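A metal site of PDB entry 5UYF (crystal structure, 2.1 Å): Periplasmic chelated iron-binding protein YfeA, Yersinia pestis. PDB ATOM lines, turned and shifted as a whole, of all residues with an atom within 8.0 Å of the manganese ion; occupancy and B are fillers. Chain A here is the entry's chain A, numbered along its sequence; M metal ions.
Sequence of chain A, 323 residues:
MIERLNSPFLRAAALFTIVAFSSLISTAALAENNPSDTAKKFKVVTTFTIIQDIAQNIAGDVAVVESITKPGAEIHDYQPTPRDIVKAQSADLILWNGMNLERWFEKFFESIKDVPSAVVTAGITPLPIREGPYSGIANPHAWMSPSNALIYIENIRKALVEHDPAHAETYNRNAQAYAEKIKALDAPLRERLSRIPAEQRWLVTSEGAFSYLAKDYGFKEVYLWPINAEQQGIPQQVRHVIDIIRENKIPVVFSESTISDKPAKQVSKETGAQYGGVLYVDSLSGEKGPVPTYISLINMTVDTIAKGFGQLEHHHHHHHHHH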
ATOM      1  N   PHE A  48      25.131 -29.729   8.637  1.00  0.00           N
ATOM      2  CA  PHE A  48      24.115 -29.079   9.466  1.00  0.00           C
ATOM      3  C   PHE A  48      23.651 -27.773   8.799  1.00  0.00           C
ATOM      4  O   PHE A  48      24.188 -27.350   7.770  1.00  0.00           O
ATOM      5  CB  PHE A  48      24.626 -28.867  10.914  1.00  0.00           C
ATOM      6  CG  PHE A  48      25.609 -27.741  11.091  1.00  0.00           C
ATOM      7  CD1 PHE A  48      26.876 -27.783  10.495  1.00  0.00           C
ATOM      8  CD2 PHE A  48      25.299 -26.655  11.897  1.00  0.00           C
ATOM      9  CE1 PHE A  48      27.790 -26.756  10.684  1.00  0.00           C
ATOM     10  CE2 PHE A  48      26.217 -25.620  12.098  1.00  0.00           C
ATOM     11  CZ  PHE A  48      27.456 -25.664  11.485  1.00  0.00           C
ATOM     12  N   GLU A  74      20.234 -31.737  17.641  1.00  0.00           N
ATOM     13  CA  GLU A  74      21.572 -31.565  18.215  1.00  0.00           C
ATOM     14  C   GLU A  74      22.642 -32.094  17.254  1.00  0.00           C
ATOM     15  O   GLU A  74      22.571 -33.245  16.816  1.00  0.00           O
ATOM     16  CB  GLU A  74      21.623 -32.290  19.554  1.00  0.00           C
ATOM     17  CG  GLU A  74      22.634 -31.707  20.525  1.00  0.00           C
ATOM     18  CD  GLU A  74      24.047 -32.055  20.101  1.00  0.00           C
ATOM     19  OE1 GLU A  74      24.376 -33.260  20.025  1.00  0.00           O
ATOM     20  OE2 GLU A  74      24.822 -31.112  19.864  1.00  0.00           O
ATOM     21  N   ILE A  75      23.639 -31.259  16.937  1.00  0.00           N
ATOM     22  CA  ILE A  75      24.532 -31.560  15.817  1.00  0.00           C
ATOM     23  C   ILE A  75      25.837 -32.229  16.257  1.00  0.00           C
ATOM     24  O   ILE A  75      26.461 -32.946  15.476  1.00  0.00           O
ATOM     25  CB  ILE A  75      24.828 -30.281  15.021  1.00  0.00           C
ATOM     26  CG1 ILE A  75      25.621 -29.272  15.872  1.00  0.00           C
ATOM     27  CG2 ILE A  75      23.546 -29.645  14.534  1.00  0.00           C
ATOM     28  CD1 ILE A  75      25.990 -27.991  15.120  1.00  0.00           C
ATOM     29  N   HIS A  76      26.265 -32.001  17.507  1.00  0.00           N
ATOM     30  CA  HIS A  76      27.579 -32.488  17.938  1.00  0.00           C
ATOM     31  C   HIS A  76      27.624 -34.011  17.985  1.00  0.00           C
ATOM     32  O   HIS A  76      28.542 -34.641  17.438  1.00  0.00           O
ATOM     33  CB  HIS A  76      27.931 -31.906  19.314  1.00  0.00           C
ATOM     34  CG  HIS A  76      28.120 -30.414  19.325  1.00  0.00           C
ATOM     35  ND1 HIS A  76      29.365 -29.829  19.398  1.00  0.00           N
ATOM     36  CD2 HIS A  76      27.225 -29.392  19.315  1.00  0.00           C
ATOM     37  CE1 HIS A  76      29.233 -28.512  19.424  1.00  0.00           C
ATOM     38  NE2 HIS A  76      27.949 -28.215  19.396  1.00  0.00           N
ATOM     39  N   LEU A 101      33.539 -30.307  15.356  1.00  0.00           N
ATOM     40  CA  LEU A 101      32.096 -30.124  15.530  1.00  0.00           C
ATOM     41  C   LEU A 101      31.376 -31.457  15.456  1.00  0.00           C
ATOM     42  O   LEU A 101      30.800 -31.917  16.451  1.00  0.00           O
ATOM     43  CB  LEU A 101      31.508 -29.168  14.496  1.00  0.00           C
ATOM     44  CG  LEU A 101      30.005 -28.905  14.623  1.00  0.00           C
ATOM     45  CD1 LEU A 101      29.634 -28.208  15.961  1.00  0.00           C
ATOM     46  CD2 LEU A 101      29.505 -28.108  13.437  1.00  0.00           C
ATOM     47  N   ASN A 139      37.492 -24.887  19.565  1.00  0.00           N
ATOM     48  CA  ASN A 139      36.054 -24.662  19.686  1.00  0.00           C
ATOM     49  C   ASN A 139      35.449 -24.638  18.279  1.00  0.00           C
ATOM     50  O   ASN A 139      35.908 -23.871  17.442  1.00  0.00           O
ATOM     51  CB  ASN A 139      35.804 -23.345  20.429  1.00  0.00           C
ATOM     52  CG  ASN A 139      34.335 -23.125  20.784  1.00  0.00           C
ATOM     53  OD1 ASN A 139      33.439 -23.411  19.983  1.00  0.00           O
ATOM     54  ND2 ASN A 139      34.103 -22.567  21.968  1.00  0.00           N
ATOM     55  N   PRO A 140      34.442 -25.473  17.986  1.00  0.00           N
ATOM     56  CA  PRO A 140      33.960 -25.559  16.590  1.00  0.00           C
ATOM     57  C   PRO A 140      33.089 -24.396  16.132  1.00  0.00           C
ATOM     58  O   PRO A 140      32.927 -24.210  14.920  1.00  0.00           O
ATOM     59  CB  PRO A 140      33.145 -26.856  16.592  1.00  0.00           C
ATOM     60  CG  PRO A 140      32.643 -26.983  18.004  1.00  0.00           C
ATOM     61  CD  PRO A 140      33.816 -26.486  18.850  1.00  0.00           C
ATOM     62  N   HIS A 141      32.563 -23.578  17.044  1.00  0.00           N
ATOM     63  CA  HIS A 141      31.511 -22.621  16.713  1.00  0.00           C
ATOM     64  C   HIS A 141      32.047 -21.355  16.047  1.00  0.00           C
ATOM     65  O   HIS A 141      31.641 -20.254  16.422  1.00  0.00           O
ATOM     66  CB  HIS A 141      30.729 -22.266  17.980  1.00  0.00           C
ATOM     67  CG  HIS A 141      30.106 -23.449  18.656  1.00  0.00           C
ATOM     68  ND1 HIS A 141      30.715 -24.124  19.694  1.00  0.00           N
ATOM     69  CD2 HIS A 141      28.954 -24.117  18.400  1.00  0.00           C
ATOM     70  CE1 HIS A 141      29.949 -25.134  20.079  1.00  0.00           C
ATOM     71  NE2 HIS A 141      28.862 -25.145  19.316  1.00  0.00           N
ATOM     72  N   TRP A 143      31.490 -19.955  13.257  1.00  0.00           N
ATOM     73  CA  TRP A 143      30.568 -19.175  12.430  1.00  0.00           C
ATOM     74  C   TRP A 143      29.837 -18.072  13.191  1.00  0.00           C
ATOM     75  O   TRP A 143      29.210 -17.217  12.554  1.00  0.00           O
ATOM     76  CB  TRP A 143      29.535 -20.137  11.786  1.00  0.00           C
ATOM     77  CG  TRP A 143      28.688 -20.840  12.804  1.00  0.00           C
ATOM     78  CD1 TRP A 143      27.556 -20.362  13.397  1.00  0.00           C
ATOM     79  CD2 TRP A 143      28.904 -22.145  13.342  1.00  0.00           C
ATOM     80  NE1 TRP A 143      27.062 -21.293  14.283  1.00  0.00           N
ATOM     81  CE2 TRP A 143      27.866 -22.405  14.263  1.00  0.00           C
ATOM     82  CE3 TRP A 143      29.889 -23.138  13.144  1.00  0.00           C
ATOM     83  CZ2 TRP A 143      27.772 -23.602  14.974  1.00  0.00           C
ATOM     84  CZ3 TRP A 143      29.794 -24.326  13.851  1.00  0.00           C
ATOM     85  CH2 TRP A 143      28.741 -24.555  14.749  1.00  0.00           C
ATOM     86  N   GLU A 207      25.591 -24.033  26.615  1.00  0.00           N
ATOM     87  CA  GLU A 207      26.826 -24.484  25.974  1.00  0.00           C
ATOM     88  C   GLU A 207      27.749 -23.278  25.790  1.00  0.00           C
ATOM     89  O   GLU A 207      27.289 -22.174  25.514  1.00  0.00           O
ATOM     90  CB  GLU A 207      26.548 -25.156  24.621  1.00  0.00           C
ATOM     91  CG  GLU A 207      27.829 -25.591  23.890  1.00  0.00           C
ATOM     92  CD  GLU A 207      27.623 -26.255  22.528  1.00  0.00           C
ATOM     93  OE1 GLU A 207      26.709 -25.869  21.738  1.00  0.00           O
ATOM     94  OE2 GLU A 207      28.420 -27.165  22.227  1.00  0.00           O
ATOM     95  N   GLY A 208      29.064 -23.502  25.944  1.00  0.00           N
ATOM     96  CA  GLY A 208      30.045 -22.468  25.658  1.00  0.00           C
ATOM     97  C   GLY A 208      30.242 -22.254  24.167  1.00  0.00           C
ATOM     98  O   GLY A 208      31.371 -22.309  23.654  1.00  0.00           O
ATOM     99  N   ALA A 209      29.141 -22.016  23.463  1.00  0.00           N
ATOM    100  CA  ALA A 209      29.109 -21.978  22.019  1.00  0.00           C
ATOM    101  C   ALA A 209      29.417 -20.606  21.454  1.00  0.00           C
ATOM    102  O   ALA A 209      29.422 -20.443  20.230  1.00  0.00           O
ATOM    103  CB  ALA A 209      27.733 -22.425  21.503  1.00  0.00           C
ATOM    104  N   PHE A 210      29.663 -19.613  22.308  1.00  0.00           N
ATOM    105  CA  PHE A 210      29.658 -18.235  21.834  1.00  0.00           C
ATOM    106  C   PHE A 210      31.033 -17.584  21.922  1.00  0.00           C
ATOM    107  O   PHE A 210      31.151 -16.367  21.770  1.00  0.00           O
ATOM    108  CB  PHE A 210      28.591 -17.455  22.600  1.00  0.00           C
ATOM    109  CG  PHE A 210      27.192 -18.003  22.390  1.00  0.00           C
ATOM    110  CD1 PHE A 210      26.423 -17.592  21.303  1.00  0.00           C
ATOM    111  CD2 PHE A 210      26.674 -18.980  23.242  1.00  0.00           C
ATOM    112  CE1 PHE A 210      25.160 -18.137  21.075  1.00  0.00           C
ATOM    113  CE2 PHE A 210      25.407 -19.506  23.030  1.00  0.00           C
ATOM    114  CZ  PHE A 210      24.642 -19.088  21.955  1.00  0.00           C
ATOM    115  N   TRP A 225      28.245 -25.687  30.388  1.00  0.00           N
ATOM    116  CA  TRP A 225      29.147 -26.747  29.966  1.00  0.00           C
ATOM    117  C   TRP A 225      29.942 -26.291  28.745  1.00  0.00           C
ATOM    118  O   TRP A 225      29.395 -25.554  27.908  1.00  0.00           O
ATOM    119  CB  TRP A 225      28.407 -28.062  29.658  1.00  0.00           C
ATOM    120  CG  TRP A 225      27.301 -27.959  28.645  1.00  0.00           C
ATOM    121  CD1 TRP A 225      27.410 -28.125  27.289  1.00  0.00           C
ATOM    122  CD2 TRP A 225      25.908 -27.716  28.912  1.00  0.00           C
ATOM    123  NE1 TRP A 225      26.173 -27.980  26.691  1.00  0.00           N
ATOM    124  CE2 TRP A 225      25.236 -27.730  27.668  1.00  0.00           C
ATOM    125  CE3 TRP A 225      25.176 -27.478  30.073  1.00  0.00           C
ATOM    126  CZ2 TRP A 225      23.861 -27.526  27.561  1.00  0.00           C
ATOM    127  CZ3 TRP A 225      23.812 -27.280  29.975  1.00  0.00           C
ATOM    128  CH2 TRP A 225      23.168 -27.302  28.727  1.00  0.00           C
ATOM    129  N   PRO A 226      31.221 -26.677  28.632  1.00  0.00           N
ATOM    130  CA  PRO A 226      32.065 -26.090  27.574  1.00  0.00           C
ATOM    131  C   PRO A 226      31.646 -26.465  26.154  1.00  0.00           C
ATOM    132  O   PRO A 226      31.766 -25.633  25.253  1.00  0.00           O
ATOM    133  CB  PRO A 226      33.468 -26.651  27.903  1.00  0.00           C
ATOM    134  CG  PRO A 226      33.212 -27.869  28.735  1.00  0.00           C
ATOM    135  CD  PRO A 226      31.967 -27.589  29.507  1.00  0.00           C
ATOM    136  N   ILE A 227      31.163 -27.683  25.940  1.00  0.00           N
ATOM    137  CA  ILE A 227      30.729 -28.125  24.616  1.00  0.00           C
ATOM    138  C   ILE A 227      29.756 -29.277  24.808  1.00  0.00           C
ATOM    139  O   ILE A 227      29.899 -30.077  25.747  1.00  0.00           O
ATOM    140  CB  ILE A 227      31.956 -28.525  23.734  1.00  0.00           C
ATOM    141  CG1 ILE A 227      31.507 -28.916  22.316  1.00  0.00           C
ATOM    142  CG2 ILE A 227      32.730 -29.660  24.359  1.00  0.00           C
ATOM    143  CD1 ILE A 227      32.641 -28.915  21.291  1.00  0.00           C
ATOM    144  N   ASN A 228      28.725 -29.326  23.957  1.00  0.00           N
ATOM    145  CA  ASN A 228      27.735 -30.386  24.049  1.00  0.00           C
ATOM    146  C   ASN A 228      28.427 -31.742  24.064  1.00  0.00           C
ATOM    147  O   ASN A 228      29.341 -31.996  23.276  1.00  0.00           O
ATOM    148  CB  ASN A 228      26.763 -30.315  22.870  1.00  0.00           C
ATOM    149  CG  ASN A 228      25.874 -29.104  22.907  1.00  0.00           C
ATOM    150  OD1 ASN A 228      25.928 -28.304  23.851  1.00  0.00           O
ATOM    151  ND2 ASN A 228      25.040 -28.944  21.888  1.00  0.00           N
ATOM    152  N   GLU A 256      20.118 -22.250  24.529  1.00  0.00           N
ATOM    153  CA  GLU A 256      20.268 -22.326  23.072  1.00  0.00           C
ATOM    154  C   GLU A 256      19.266 -23.324  22.500  1.00  0.00           C
ATOM    155  O   GLU A 256      18.747 -24.181  23.213  1.00  0.00           O
ATOM    156  CB  GLU A 256      21.692 -22.710  22.684  1.00  0.00           C
ATOM    157  CG  GLU A 256      22.761 -21.782  23.253  1.00  0.00           C
ATOM    158  CD  GLU A 256      23.195 -22.192  24.644  1.00  0.00           C
ATOM    159  OE1 GLU A 256      23.591 -23.367  24.811  1.00  0.00           O
ATOM    160  OE2 GLU A 256      23.100 -21.372  25.587  1.00  0.00           O
ATOM    161  N   THR A 258      19.032 -25.990  20.455  1.00  0.00           N
ATOM    162  CA  THR A 258      19.030 -27.443  20.330  1.00  0.00           C
ATOM    163  C   THR A 258      19.209 -28.177  21.652  1.00  0.00           C
ATOM    164  O   THR A 258      19.250 -29.416  21.649  1.00  0.00           O
ATOM    165  CB  THR A 258      20.098 -27.931  19.337  1.00  0.00           C
ATOM    166  OG1 THR A 258      21.407 -27.729  19.893  1.00  0.00           O
ATOM    167  CG2 THR A 258      19.959 -27.195  18.026  1.00  0.00           C
ATOM    168  N   ILE A 259      19.310 -27.480  22.771  1.00  0.00           N
ATOM    169  CA  ILE A 259      19.514 -28.149  24.056  1.00  0.00           C
ATOM    170  C   ILE A 259      18.375 -27.754  25.006  1.00  0.00           C
ATOM    171  O   ILE A 259      17.516 -26.950  24.648  1.00  0.00           O
ATOM    172  CB  ILE A 259      20.902 -27.819  24.630  1.00  0.00           C
ATOM    173  CG1 ILE A 259      21.181 -26.314  24.529  1.00  0.00           C
ATOM    174  CG2 ILE A 259      21.972 -28.570  23.853  1.00  0.00           C
ATOM    175  CD1 ILE A 259      20.695 -25.510  25.762  1.00  0.00           C
ATOM    176  N   VAL A 281      22.457 -20.938  17.669  1.00  0.00           N
ATOM    177  CA  VAL A 281      23.871 -21.100  17.330  1.00  0.00           C
ATOM    178  C   VAL A 281      24.105 -22.402  16.558  1.00  0.00           C
ATOM    179  O   VAL A 281      24.726 -22.405  15.503  1.00  0.00           O
ATOM    180  CB  VAL A 281      24.773 -21.021  18.577  1.00  0.00           C
ATOM    181  CG1 VAL A 281      24.237 -21.892  19.712  1.00  0.00           C
ATOM    182  CG2 VAL A 281      26.229 -21.404  18.221  1.00  0.00           C
ATOM    183  N   ASP A 282      23.585 -23.519  17.069  1.00  0.00           N
ATOM    184  CA  ASP A 282      23.854 -24.799  16.409  1.00  0.00           C
ATOM    185  C   ASP A 282      22.861 -25.135  15.292  1.00  0.00           C
ATOM    186  O   ASP A 282      23.125 -26.055  14.512  1.00  0.00           O
ATOM    187  CB  ASP A 282      23.879 -25.941  17.435  1.00  0.00           C
ATOM    188  CG  ASP A 282      25.189 -25.989  18.251  1.00  0.00           C
ATOM    189  OD1 ASP A 282      26.106 -25.184  18.010  1.00  0.00           O
ATOM    190  OD2 ASP A 282      25.317 -26.842  19.140  1.00  0.00           O
ATOM    191  N   SER A 283      21.719 -24.450  15.211  1.00  0.00           N
ATOM    192  CA  SER A 283      20.739 -24.770  14.183  1.00  0.00           C
ATOM    193  C   SER A 283      19.976 -23.517  13.791  1.00  0.00           C
ATOM    194  O   SER A 283      19.706 -22.639  14.624  1.00  0.00           O
ATOM    195  CB  SER A 283      19.740 -25.845  14.653  1.00  0.00           C
ATOM    196  OG  SER A 283      18.827 -26.189  13.602  1.00  0.00           O
HETATM  197 MN    MN M   1      27.266 -26.437  19.858  1.00  0.00          MN
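Asn 228 touches the manganese ion.
Five residues have an atom within 4 Å of the manganese ion: His 76, His 141, Glu 207, Asn 228 and Asp 282.
The nearest printed residue that does not touch the manganese ion is Ala 209 (4.4 Å).
The manganese ion is bound by a ring nitrogen (NE2) of His 76 (2.0 Å), the side-chain carboxylate (OE1) of Glu 207 (2.0 Å), the side-chain carboxylate (OD2) of Asp 282 (2.1 Å), a ring nitrogen (NE2) of His 141 (2.1 Å) and the side-chain carboxylate (OD1) of Asp 282 (2.5 Å).
The manganese ion has five donor atoms within binding distance.
Slightly farther from the manganese ion lies OE2 of Glu 207 (2.7 Å).
N of His 76 lies within hydrogen-bond range of OE2 of Glu 74, 2.9 Å away.
The backbone NH (N) of Asn 228 lies within hydrogen-bond range of the side-chain carboxylate (OE2) of Glu 207 (2.8 Å).
The side-chain carboxylate of Glu 256 lies within hydrogen-bond range of the backbone NH of Glu 207, at 2.8 Å.
OD2 of Asp 282 lies close to ND2 of Asn 228 (3.5 Å).
A ring nitrogen (ND1) of His 141 sits at hydrogen-bond distance from the side-chain amide oxygen (OD1) of Asn 139, 2.8 Å away.
The side-chain carboxylate (OE2) of Glu 74 is in hydrogen-bond range of the side-chain amide nitrogen (ND2) of Asn 228, at 3.0 Å.
OD1 of Asn 228 sits at hydrogen-bond distance from NE1 of Trp 225 (2.9 Å).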
